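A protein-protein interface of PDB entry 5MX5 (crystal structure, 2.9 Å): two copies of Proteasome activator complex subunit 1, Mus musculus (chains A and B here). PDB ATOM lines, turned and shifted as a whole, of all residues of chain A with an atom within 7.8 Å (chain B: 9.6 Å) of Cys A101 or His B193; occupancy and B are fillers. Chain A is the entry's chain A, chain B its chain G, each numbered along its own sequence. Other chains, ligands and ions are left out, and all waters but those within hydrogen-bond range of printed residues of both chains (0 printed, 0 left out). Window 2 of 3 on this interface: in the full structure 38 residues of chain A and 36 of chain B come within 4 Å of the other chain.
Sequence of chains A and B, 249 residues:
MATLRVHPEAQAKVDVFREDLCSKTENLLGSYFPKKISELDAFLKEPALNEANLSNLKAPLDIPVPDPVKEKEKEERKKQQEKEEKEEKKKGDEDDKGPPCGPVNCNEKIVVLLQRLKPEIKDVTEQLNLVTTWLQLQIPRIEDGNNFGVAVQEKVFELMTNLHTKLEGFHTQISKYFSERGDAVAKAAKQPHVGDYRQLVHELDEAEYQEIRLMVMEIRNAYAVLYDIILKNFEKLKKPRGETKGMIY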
ATOM      1  N   LEU A  61       7.776  24.669  35.991  1.00  0.00           N
ATOM      2  CA  LEU A  61       8.282  24.985  34.654  1.00  0.00           C
ATOM      3  C   LEU A  61       8.815  26.421  34.664  1.00  0.00           C
ATOM      4  O   LEU A  61       8.192  27.342  34.125  1.00  0.00           O
ATOM      5  CB  LEU A  61       7.174  24.790  33.606  1.00  0.00           C
ATOM      6  CG  LEU A  61       7.533  24.931  32.122  1.00  0.00           C
ATOM      7  CD1 LEU A  61       8.563  23.894  31.698  1.00  0.00           C
ATOM      8  CD2 LEU A  61       6.280  24.817  31.267  1.00  0.00           C
ATOM      9  N   ASP A  62       9.976  26.592  35.295  1.00  0.00           N
ATOM     10  CA  ASP A  62      10.579  27.913  35.500  1.00  0.00           C
ATOM     11  C   ASP A  62      11.221  28.449  34.219  1.00  0.00           C
ATOM     12  O   ASP A  62      12.412  28.240  33.969  1.00  0.00           O
ATOM     13  CB  ASP A  62      11.610  27.869  36.639  1.00  0.00           C
ATOM     14  CG  ASP A  62      10.987  27.548  37.995  1.00  0.00           C
ATOM     15  OD1 ASP A  62      11.700  27.672  39.013  1.00  0.00           O
ATOM     16  OD2 ASP A  62       9.795  27.172  38.051  1.00  0.00           O
ATOM     17  N   ILE A  63      10.404  29.126  33.411  1.00  0.00           N
ATOM     18  CA  ILE A  63      10.844  29.812  32.192  1.00  0.00           C
ATOM     19  C   ILE A  63      10.361  31.266  32.295  1.00  0.00           C
ATOM     20  O   ILE A  63       9.212  31.498  32.683  1.00  0.00           O
ATOM     21  CB  ILE A  63      10.271  29.134  30.921  1.00  0.00           C
ATOM     22  CG1 ILE A  63      10.693  27.656  30.866  1.00  0.00           C
ATOM     23  CG2 ILE A  63      10.744  29.838  29.650  1.00  0.00           C
ATOM     24  CD1 ILE A  63      10.053  26.862  29.746  1.00  0.00           C
ATOM     25  N   PRO A  64      11.226  32.249  31.956  1.00  0.00           N
ATOM     26  CA  PRO A  64      10.819  33.655  32.076  1.00  0.00           C
ATOM     27  C   PRO A  64       9.802  34.088  31.015  1.00  0.00           C
ATOM     28  O   PRO A  64       9.988  33.806  29.829  1.00  0.00           O
ATOM     29  CB  PRO A  64      12.137  34.417  31.902  1.00  0.00           C
ATOM     30  CG  PRO A  64      12.976  33.520  31.064  1.00  0.00           C
ATOM     31  CD  PRO A  64      12.626  32.128  31.504  1.00  0.00           C
ATOM     32  N   PRO A 100      17.672  30.689  27.441  1.00  0.00           N
ATOM     33  CA  PRO A 100      18.303  31.496  28.476  1.00  0.00           C
ATOM     34  C   PRO A 100      17.497  31.452  29.784  1.00  0.00           C
ATOM     35  O   PRO A 100      17.105  32.495  30.320  1.00  0.00           O
ATOM     36  CB  PRO A 100      18.316  32.891  27.843  1.00  0.00           C
ATOM     37  CG  PRO A 100      17.069  32.921  27.018  1.00  0.00           C
ATOM     38  CD  PRO A 100      16.786  31.500  26.587  1.00  0.00           C
ATOM     39  N   CYS A 101      17.267  30.237  30.284  1.00  0.00           N
ATOM     40  CA  CYS A 101      16.444  30.004  31.477  1.00  0.00           C
ATOM     41  C   CYS A 101      17.091  28.991  32.423  1.00  0.00           C
ATOM     42  O   CYS A 101      18.111  28.377  32.093  1.00  0.00           O
ATOM     43  CB  CYS A 101      15.052  29.512  31.065  1.00  0.00           C
ATOM     44  SG  CYS A 101      15.024  27.874  30.298  1.00  0.00           S
ATOM     45  N   GLY A 102      16.483  28.822  33.597  1.00  0.00           N
ATOM     46  CA  GLY A 102      16.952  27.863  34.599  1.00  0.00           C
ATOM     47  C   GLY A 102      16.685  26.413  34.217  1.00  0.00           C
ATOM     48  O   GLY A 102      16.030  26.146  33.204  1.00  0.00           O
ATOM     49  N   PRO A 103      17.182  25.463  35.033  1.00  0.00           N
ATOM     50  CA  PRO A 103      17.070  24.038  34.713  1.00  0.00           C
ATOM     51  C   PRO A 103      15.660  23.479  34.937  1.00  0.00           C
ATOM     52  O   PRO A 103      15.155  23.519  36.062  1.00  0.00           O
ATOM     53  CB  PRO A 103      18.072  23.388  35.671  1.00  0.00           C
ATOM     54  CG  PRO A 103      18.107  24.299  36.850  1.00  0.00           C
ATOM     55  CD  PRO A 103      17.845  25.686  36.332  1.00  0.00           C
ATOM     56  N   VAL A 104      15.047  22.968  33.868  1.00  0.00           N
ATOM     57  CA  VAL A 104      13.714  22.359  33.933  1.00  0.00           C
ATOM     58  C   VAL A 104      13.868  20.861  34.214  1.00  0.00           C
ATOM     59  O   VAL A 104      14.242  20.091  33.326  1.00  0.00           O
ATOM     60  CB  VAL A 104      12.916  22.577  32.623  1.00  0.00           C
ATOM     61  CG1 VAL A 104      11.490  22.049  32.766  1.00  0.00           C
ATOM     62  CG2 VAL A 104      12.905  24.052  32.239  1.00  0.00           C
ATOM     63  N   ASN A 105      13.580  20.462  35.453  1.00  0.00           N
ATOM     64  CA  ASN A 105      13.704  19.062  35.875  1.00  0.00           C
ATOM     65  C   ASN A 105      12.500  18.232  35.438  1.00  0.00           C
ATOM     66  O   ASN A 105      11.476  18.773  35.010  1.00  0.00           O
ATOM     67  CB  ASN A 105      13.871  18.970  37.396  1.00  0.00           C
ATOM     68  CG  ASN A 105      15.181  19.563  37.878  1.00  0.00           C
ATOM     69  OD1 ASN A 105      15.194  20.510  38.665  1.00  0.00           O
ATOM     70  ND2 ASN A 105      16.293  19.009  37.405  1.00  0.00           N
ATOM     71  N   CYS A 106      12.639  16.913  35.552  1.00  0.00           N
ATOM     72  CA  CYS A 106      11.558  15.974  35.251  1.00  0.00           C
ATOM     73  C   CYS A 106      10.490  16.002  36.343  1.00  0.00           C
ATOM     74  O   CYS A 106      10.742  16.458  37.463  1.00  0.00           O
ATOM     75  CB  CYS A 106      12.104  14.550  35.111  1.00  0.00           C
ATOM     76  SG  CYS A 106      13.415  14.366  33.881  1.00  0.00           S
ATOM     77  N   GLY A 182      10.531  16.354  26.422  1.00  0.00           N
ATOM     78  CA  GLY A 182      11.770  17.069  26.114  1.00  0.00           C
ATOM     79  C   GLY A 182      11.622  18.066  24.976  1.00  0.00           C
ATOM     80  O   GLY A 182      12.126  19.187  25.064  1.00  0.00           O
ATOM     81  N   VAL A 185       9.278  20.995  26.238  1.00  0.00           N
ATOM     82  CA  VAL A 185      10.046  21.896  27.109  1.00  0.00           C
ATOM     83  C   VAL A 185      11.086  22.682  26.298  1.00  0.00           C
ATOM     84  O   VAL A 185      11.320  23.862  26.573  1.00  0.00           O
ATOM     85  CB  VAL A 185      10.732  21.128  28.274  1.00  0.00           C
ATOM     86  CG1 VAL A 185      11.650  22.040  29.083  1.00  0.00           C
ATOM     87  CG2 VAL A 185       9.690  20.508  29.199  1.00  0.00           C
ATOM     88  N   ALA A 186      11.703  22.027  25.313  1.00  0.00           N
ATOM     89  CA  ALA A 186      12.655  22.684  24.407  1.00  0.00           C
ATOM     90  C   ALA A 186      11.989  23.785  23.577  1.00  0.00           C
ATOM     91  O   ALA A 186      12.529  24.884  23.461  1.00  0.00           O
ATOM     92  CB  ALA A 186      13.318  21.663  23.492  1.00  0.00           C
ATOM     93  N   LYS A 187      10.823  23.479  23.007  1.00  0.00           N
ATOM     94  CA  LYS A 187      10.035  24.465  22.249  1.00  0.00           C
ATOM     95  C   LYS A 187       9.505  25.601  23.130  1.00  0.00           C
ATOM     96  O   LYS A 187       9.449  26.751  22.691  1.00  0.00           O
ATOM     97  CB  LYS A 187       8.869  23.792  21.514  1.00  0.00           C
ATOM     98  CG  LYS A 187       9.285  23.020  20.273  1.00  0.00           C
ATOM     99  CD  LYS A 187       8.119  22.245  19.686  1.00  0.00           C
ATOM    100  CE  LYS A 187       8.454  21.696  18.309  1.00  0.00           C
ATOM    101  NZ  LYS A 187       7.384  20.800  17.795  1.00  0.00           N
ATOM    102  N   ALA A 188       9.110  25.269  24.361  1.00  0.00           N
ATOM    103  CA  ALA A 188       8.664  26.268  25.340  1.00  0.00           C
ATOM    104  C   ALA A 188       9.789  27.224  25.753  1.00  0.00           C
ATOM    105  O   ALA A 188       9.545  28.414  25.956  1.00  0.00           O
ATOM    106  CB  ALA A 188       8.079  25.583  26.568  1.00  0.00           C
ATOM    107  N   ALA A 189      11.008  26.698  25.877  1.00  0.00           N
ATOM    108  CA  ALA A 189      12.184  27.501  26.239  1.00  0.00           C
ATOM    109  C   ALA A 189      12.648  28.410  25.095  1.00  0.00           C
ATOM    110  O   ALA A 189      12.961  29.581  25.324  1.00  0.00           O
ATOM    111  CB  ALA A 189      13.325  26.599  26.688  1.00  0.00           C
ATOM    112  N   LYS A 190      12.702  27.865  23.879  1.00  0.00           N
ATOM    113  CA  LYS A 190      13.075  28.636  22.679  1.00  0.00           C
ATOM    114  C   LYS A 190      12.097  29.772  22.374  1.00  0.00           C
ATOM    115  O   LYS A 190      12.517  30.863  21.983  1.00  0.00           O
ATOM    116  CB  LYS A 190      13.174  27.733  21.444  1.00  0.00           C
ATOM    117  CG  LYS A 190      14.395  26.829  21.402  1.00  0.00           C
ATOM    118  CD  LYS A 190      14.477  26.108  20.064  1.00  0.00           C
ATOM    119  CE  LYS A 190      15.327  24.851  20.143  1.00  0.00           C
ATOM    120  NZ  LYS A 190      15.411  24.158  18.827  1.00  0.00           N
ATOM    121  N   PRO A 192       9.299  31.436  24.535  1.00  0.00           N
ATOM    122  CA  PRO A 192       8.520  31.632  25.769  1.00  0.00           C
ATOM    123  C   PRO A 192       7.180  32.356  25.571  1.00  0.00           C
ATOM    124  O   PRO A 192       6.263  32.166  26.373  1.00  0.00           O
ATOM    125  CB  PRO A 192       9.457  32.477  26.654  1.00  0.00           C
ATOM    126  CG  PRO A 192      10.804  32.387  26.026  1.00  0.00           C
ATOM    127  CD  PRO A 192      10.541  32.229  24.563  1.00  0.00           C
ATOM    128  N   ILE B  63      27.688  16.512  30.969  1.00  0.00           N
ATOM    129  CA  ILE B  63      27.374  17.761  30.270  1.00  0.00           C
ATOM    130  C   ILE B  63      27.236  18.851  31.342  1.00  0.00           C
ATOM    131  O   ILE B  63      26.570  18.626  32.357  1.00  0.00           O
ATOM    132  CB  ILE B  63      26.072  17.633  29.438  1.00  0.00           C
ATOM    133  CG1 ILE B  63      26.203  16.481  28.429  1.00  0.00           C
ATOM    134  CG2 ILE B  63      25.745  18.935  28.705  1.00  0.00           C
ATOM    135  CD1 ILE B  63      25.000  16.284  27.529  1.00  0.00           C
ATOM    136  N   PRO B  64      27.863  20.030  31.129  1.00  0.00           N
ATOM    137  CA  PRO B  64      27.828  21.078  32.156  1.00  0.00           C
ATOM    138  C   PRO B  64      26.449  21.723  32.308  1.00  0.00           C
ATOM    139  O   PRO B  64      25.810  22.053  31.306  1.00  0.00           O
ATOM    140  CB  PRO B  64      28.848  22.101  31.644  1.00  0.00           C
ATOM    141  CG  PRO B  64      28.831  21.931  30.166  1.00  0.00           C
ATOM    142  CD  PRO B  64      28.628  20.461  29.941  1.00  0.00           C
ATOM    143  N   VAL B  65      26.008  21.892  33.555  1.00  0.00           N
ATOM    144  CA  VAL B  65      24.706  22.510  33.850  1.00  0.00           C
ATOM    145  C   VAL B  65      24.755  24.026  33.590  1.00  0.00           C
ATOM    146  O   VAL B  65      25.814  24.641  33.754  1.00  0.00           O
ATOM    147  CB  VAL B  65      24.227  22.230  35.305  1.00  0.00           C
ATOM    148  CG1 VAL B  65      24.183  20.730  35.579  1.00  0.00           C
ATOM    149  CG2 VAL B  65      25.084  22.958  36.344  1.00  0.00           C
ATOM    150  N   PRO B  66      23.617  24.630  33.185  1.00  0.00           N
ATOM    151  CA  PRO B  66      23.608  26.060  32.873  1.00  0.00           C
ATOM    152  C   PRO B  66      23.563  26.929  34.129  1.00  0.00           C
ATOM    153  O   PRO B  66      24.538  27.614  34.438  1.00  0.00           O
ATOM    154  CB  PRO B  66      22.324  26.224  32.057  1.00  0.00           C
ATOM    155  CG  PRO B  66      21.408  25.191  32.611  1.00  0.00           C
ATOM    156  CD  PRO B  66      22.274  24.034  33.034  1.00  0.00           C
ATOM    157  N   PRO B  99      26.793  25.488  22.995  1.00  0.00           N
ATOM    158  CA  PRO B  99      27.614  25.179  24.165  1.00  0.00           C
ATOM    159  C   PRO B  99      28.726  24.169  23.837  1.00  0.00           C
ATOM    160  O   PRO B  99      28.436  23.141  23.219  1.00  0.00           O
ATOM    161  CB  PRO B  99      26.607  24.573  25.153  1.00  0.00           C
ATOM    162  CG  PRO B  99      25.286  25.125  24.740  1.00  0.00           C
ATOM    163  CD  PRO B  99      25.357  25.272  23.249  1.00  0.00           C
ATOM    164  N   LYS B 187      20.603  16.510  21.594  1.00  0.00           N
ATOM    165  CA  LYS B 187      19.629  17.455  22.156  1.00  0.00           C
ATOM    166  C   LYS B 187      19.958  17.851  23.600  1.00  0.00           C
ATOM    167  O   LYS B 187      19.759  19.005  23.981  1.00  0.00           O
ATOM    168  CB  LYS B 187      18.207  16.884  22.073  1.00  0.00           C
ATOM    169  CG  LYS B 187      17.644  16.851  20.659  1.00  0.00           C
ATOM    170  CD  LYS B 187      16.367  16.031  20.579  1.00  0.00           C
ATOM    171  CE  LYS B 187      15.677  16.202  19.235  1.00  0.00           C
ATOM    172  NZ  LYS B 187      14.507  15.290  19.089  1.00  0.00           N
ATOM    173  N   ALA B 188      20.456  16.899  24.392  1.00  0.00           N
ATOM    174  CA  ALA B 188      20.855  17.157  25.785  1.00  0.00           C
ATOM    175  C   ALA B 188      22.033  18.130  25.895  1.00  0.00           C
ATOM    176  O   ALA B 188      22.066  18.965  26.802  1.00  0.00           O
ATOM    177  CB  ALA B 188      21.191  15.853  26.493  1.00  0.00           C
ATOM    178  N   ALA B 189      22.995  18.009  24.980  1.00  0.00           N
ATOM    179  CA  ALA B 189      24.153  18.908  24.930  1.00  0.00           C
ATOM    180  C   ALA B 189      23.768  20.306  24.439  1.00  0.00           C
ATOM    181  O   ALA B 189      24.194  21.307  25.018  1.00  0.00           O
ATOM    182  CB  ALA B 189      25.242  18.319  24.043  1.00  0.00           C
ATOM    183  N   LYS B 190      22.972  20.362  23.370  1.00  0.00           N
ATOM    184  CA  LYS B 190      22.465  21.633  22.830  1.00  0.00           C
ATOM    185  C   LYS B 190      21.461  22.329  23.757  1.00  0.00           C
ATOM    186  O   LYS B 190      21.356  23.558  23.735  1.00  0.00           O
ATOM    187  CB  LYS B 190      21.830  21.423  21.450  1.00  0.00           C
ATOM    188  CG  LYS B 190      22.836  21.078  20.362  1.00  0.00           C
ATOM    189  CD  LYS B 190      22.147  20.631  19.084  1.00  0.00           C
ATOM    190  CE  LYS B 190      23.160  20.193  18.037  1.00  0.00           C
ATOM    191  NZ  LYS B 190      22.513  19.531  16.870  1.00  0.00           N
ATOM    192  N   GLN B 191      20.734  21.547  24.560  1.00  0.00           N
ATOM    193  CA  GLN B 191      19.771  22.070  25.533  1.00  0.00           C
ATOM    194  C   GLN B 191      20.090  21.505  26.930  1.00  0.00           C
ATOM    195  O   GLN B 191      19.444  20.552  27.374  1.00  0.00           O
ATOM    196  CB  GLN B 191      18.334  21.704  25.118  1.00  0.00           C
ATOM    197  CG  GLN B 191      17.938  22.056  23.686  1.00  0.00           C
ATOM    198  CD  GLN B 191      17.613  23.527  23.498  1.00  0.00           C
ATOM    199  OE1 GLN B 191      18.436  24.399  23.772  1.00  0.00           O
ATOM    200  NE2 GLN B 191      16.408  23.809  23.016  1.00  0.00           N
ATOM    201  N   PRO B 192      21.103  22.075  27.623  1.00  0.00           N
ATOM    202  CA  PRO B 192      21.458  21.594  28.971  1.00  0.00           C
ATOM    203  C   PRO B 192      20.360  21.801  30.022  1.00  0.00           C
ATOM    204  O   PRO B 192      20.174  20.947  30.891  1.00  0.00           O
ATOM    205  CB  PRO B 192      22.701  22.424  29.334  1.00  0.00           C
ATOM    206  CG  PRO B 192      23.212  22.963  28.045  1.00  0.00           C
ATOM    207  CD  PRO B 192      22.002  23.163  27.190  1.00  0.00           C
ATOM    208  N   HIS B 193      19.668  22.936  29.939  1.00  0.00           N
ATOM    209  CA  HIS B 193      18.526  23.252  30.818  1.00  0.00           C
ATOM    210  C   HIS B 193      17.378  22.227  30.802  1.00  0.00           C
ATOM    211  O   HIS B 193      16.700  22.053  31.818  1.00  0.00           O
ATOM    212  CB  HIS B 193      17.977  24.663  30.526  1.00  0.00           C
ATOM    213  CG  HIS B 193      17.480  24.856  29.124  1.00  0.00           C
ATOM    214  ND1 HIS B 193      18.307  25.230  28.085  1.00  0.00           N
ATOM    215  CD2 HIS B 193      16.238  24.748  28.594  1.00  0.00           C
ATOM    216  CE1 HIS B 193      17.599  25.329  26.974  1.00  0.00           C
ATOM    217  NE2 HIS B 193      16.341  25.043  27.255  1.00  0.00           N
ATOM    218  N   VAL B 194      17.166  21.553  29.670  1.00  0.00           N
ATOM    219  CA  VAL B 194      16.092  20.558  29.543  1.00  0.00           C
ATOM    220  C   VAL B 194      16.538  19.239  30.188  1.00  0.00           C
ATOM    221  O   VAL B 194      17.348  18.503  29.620  1.00  0.00           O
ATOM    222  CB  VAL B 194      15.678  20.327  28.068  1.00  0.00           C
ATOM    223  CG1 VAL B 194      14.517  19.341  27.978  1.00  0.00           C
ATOM    224  CG2 VAL B 194      15.298  21.649  27.407  1.00  0.00           C
ATOM    225  N   GLY B 195      16.001  18.954  31.374  1.00  0.00           N
ATOM    226  CA  GLY B 195      16.355  17.754  32.135  1.00  0.00           C
ATOM    227  C   GLY B 195      15.804  16.438  31.603  1.00  0.00           C
ATOM    228  O   GLY B 195      16.311  15.374  31.958  1.00  0.00           O
ATOM    229  N   ASP B 196      14.765  16.504  30.768  1.00  0.00           N
ATOM    230  CA  ASP B 196      14.143  15.301  30.191  1.00  0.00           C
ATOM    231  C   ASP B 196      15.021  14.597  29.156  1.00  0.00           C
ATOM    232  O   ASP B 196      14.970  13.370  29.043  1.00  0.00           O
ATOM    233  CB  ASP B 196      12.789  15.639  29.564  1.00  0.00           C
ATOM    234  CG  ASP B 196      11.756  16.040  30.594  1.00  0.00           C
ATOM    235  OD1 ASP B 196      11.303  17.203  30.563  1.00  0.00           O
ATOM    236  OD2 ASP B 196      11.403  15.195  31.444  1.00  0.00           O
ATOM    237  N   TYR B 197      15.809  15.365  28.400  1.00  0.00           N
ATOM    238  CA  TYR B 197      16.761  14.792  27.439  1.00  0.00           C
ATOM    239  C   TYR B 197      17.860  13.977  28.126  1.00  0.00           C
ATOM    240  O   TYR B 197      18.336  12.991  27.563  1.00  0.00           O
ATOM    241  CB  TYR B 197      17.407  15.882  26.568  1.00  0.00           C
ATOM    242  CG  TYR B 197      16.484  16.574  25.577  1.00  0.00           C
ATOM    243  CD1 TYR B 197      15.578  15.849  24.793  1.00  0.00           C
ATOM    244  CD2 TYR B 197      16.551  17.957  25.390  1.00  0.00           C
ATOM    245  CE1 TYR B 197      14.749  16.487  23.880  1.00  0.00           C
ATOM    246  CE2 TYR B 197      15.728  18.601  24.475  1.00  0.00           C
ATOM    247  CZ  TYR B 197      14.831  17.863  23.723  1.00  0.00           C
ATOM    248  OH  TYR B 197      14.017  18.499  22.816  1.00  0.00           O
ATOM    249  N   ARG B 198      18.262  14.394  29.327  1.00  0.00           N
ATOM    250  CA  ARG B 198      19.211  13.628  30.146  1.00  0.00           C
ATOM    251  C   ARG B 198      18.581  12.315  30.605  1.00  0.00           C
ATOM    252  O   ARG B 198      19.203  11.256  30.513  1.00  0.00           O
ATOM    253  CB  ARG B 198      19.659  14.429  31.373  1.00  0.00           C
ATOM    254  CG  ARG B 198      20.453  15.689  31.059  1.00  0.00           C
ATOM    255  CD  ARG B 198      20.486  16.629  32.254  1.00  0.00           C
ATOM    256  NE  ARG B 198      21.184  17.879  31.955  1.00  0.00           N
ATOM    257  CZ  ARG B 198      22.511  18.038  31.908  1.00  0.00           C
ATOM    258  NH1 ARG B 198      23.345  17.021  32.132  1.00  0.00           N
ATOM    259  NH2 ARG B 198      23.014  19.238  31.625  1.00  0.00           N
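Positions printed for both chains: 63, 64, 187, 188, 189, 190 and 192.
Of the 16 pairs that touch across the chains among the printed residues, none has its exchanged pair printed and touching as well.
Cys A101 touches just one residue of chain B: His B193 (3.8 Å).
Of chain B, only His B193 comes within 4 Å of Gly A102.
Printed residues of chain B within 4 Å of Pro A103: His B193 (3.5 Å).
Printed residues of chain B within 4 Å of Cys A106: Gly B195 (3.6 Å) and Asp B196 (3.3 Å).
Printed residues of chain A within 4 Å of Gln B191: Ala A186 (3.8 Å) and Lys A190 (3.2 Å).
His B193 touches just these residues of chain A: Cys A101, Gly A102, Pro A103, Val A104 and Ala A189.
Printed residues of chain A within 4 Å of Val B194: Val A104 and Gly A182.
Of the printed residues of chain A, Asp B196 touches Cys A106 (3.3 Å), Gly A182 (3.9 Å) and Val A185 (3.9 Å).
The nearest residue of chain B that does not touch Cys A101 is Pro B66 (4.6 Å).
The nearest residue of chain A that does not touch His B193 is Asn A105 (5.0 Å).
The nearest printed residue of chain A that does not touch Gly B195 is Asn A105 (4.8 Å).
The backbone NH (N) of Val A104 lies within hydrogen-bond range of the backbone carbonyl oxygen (O) of His B193, at 2.8 Å.
The backbone carbonyl oxygen of Val A104 is in hydrogen-bond range of the backbone NH of Gly B195 (2.9 Å).
SG of Cys A106 sits at hydrogen-bond distance from O of Gly B195, 3.6 Å away.
OD2 of Asp B196 is in hydrogen-bond range of SG of Cys A106.
The side-chain hydroxyl of Tyr B197 is in hydrogen-bond range of the backbone carbonyl oxygen of Gly A182 (3.0 Å).
Printed residues of chain A that touch a printed residue of chain B: Cys A101, Gly A102, Pro A103, Val A104, Cys A106, Gly A182, Val A185, Ala A186, Ala A189 and Lys A190.
Printed residues of chain B that touch a printed residue of chain A: Gln B191, His B193, Val B194, Gly B195, Asp B196 and Tyr B197.
Hydrophobic or aromatic side chains of chain B within 4 Å of the printed part of chain A: His B193, Val B194 and Tyr B197.
Along chain B the printed residues that touch a printed residue of chain A span positions 191 to 197.
Among the printed residues, 16 pairs touch across the chains.
Among the printed residues, no Asp or Glu carboxylate lies within 4 Å of a Lys or Arg side-chain nitrogen of the other chain.
Cys A101 touches His B193.
O of Gly A102 touches CB of His B193, 3.6 Å away.
His B193 touches Pro A103 (O to CA, 3.5 Å).
Val A104 touches Val B194 (O to C, 3.98 Å).
CG1 of Val B194 touches O of Gly A182, at 3.8 Å.
Gly A182 touches Asp B196 (CA to CB, 3.9 Å).
CG2 of Val A185 touches OD1 of Asp B196 (3.9 Å).
Ala A186 touches Gln B191 (CB to NE2, 3.8 Å).
CB of Ala A186 touches OH of Tyr B197, at 3.3 Å.
Ala A189 touches His B193 (CB to NE2, 3.4 Å).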
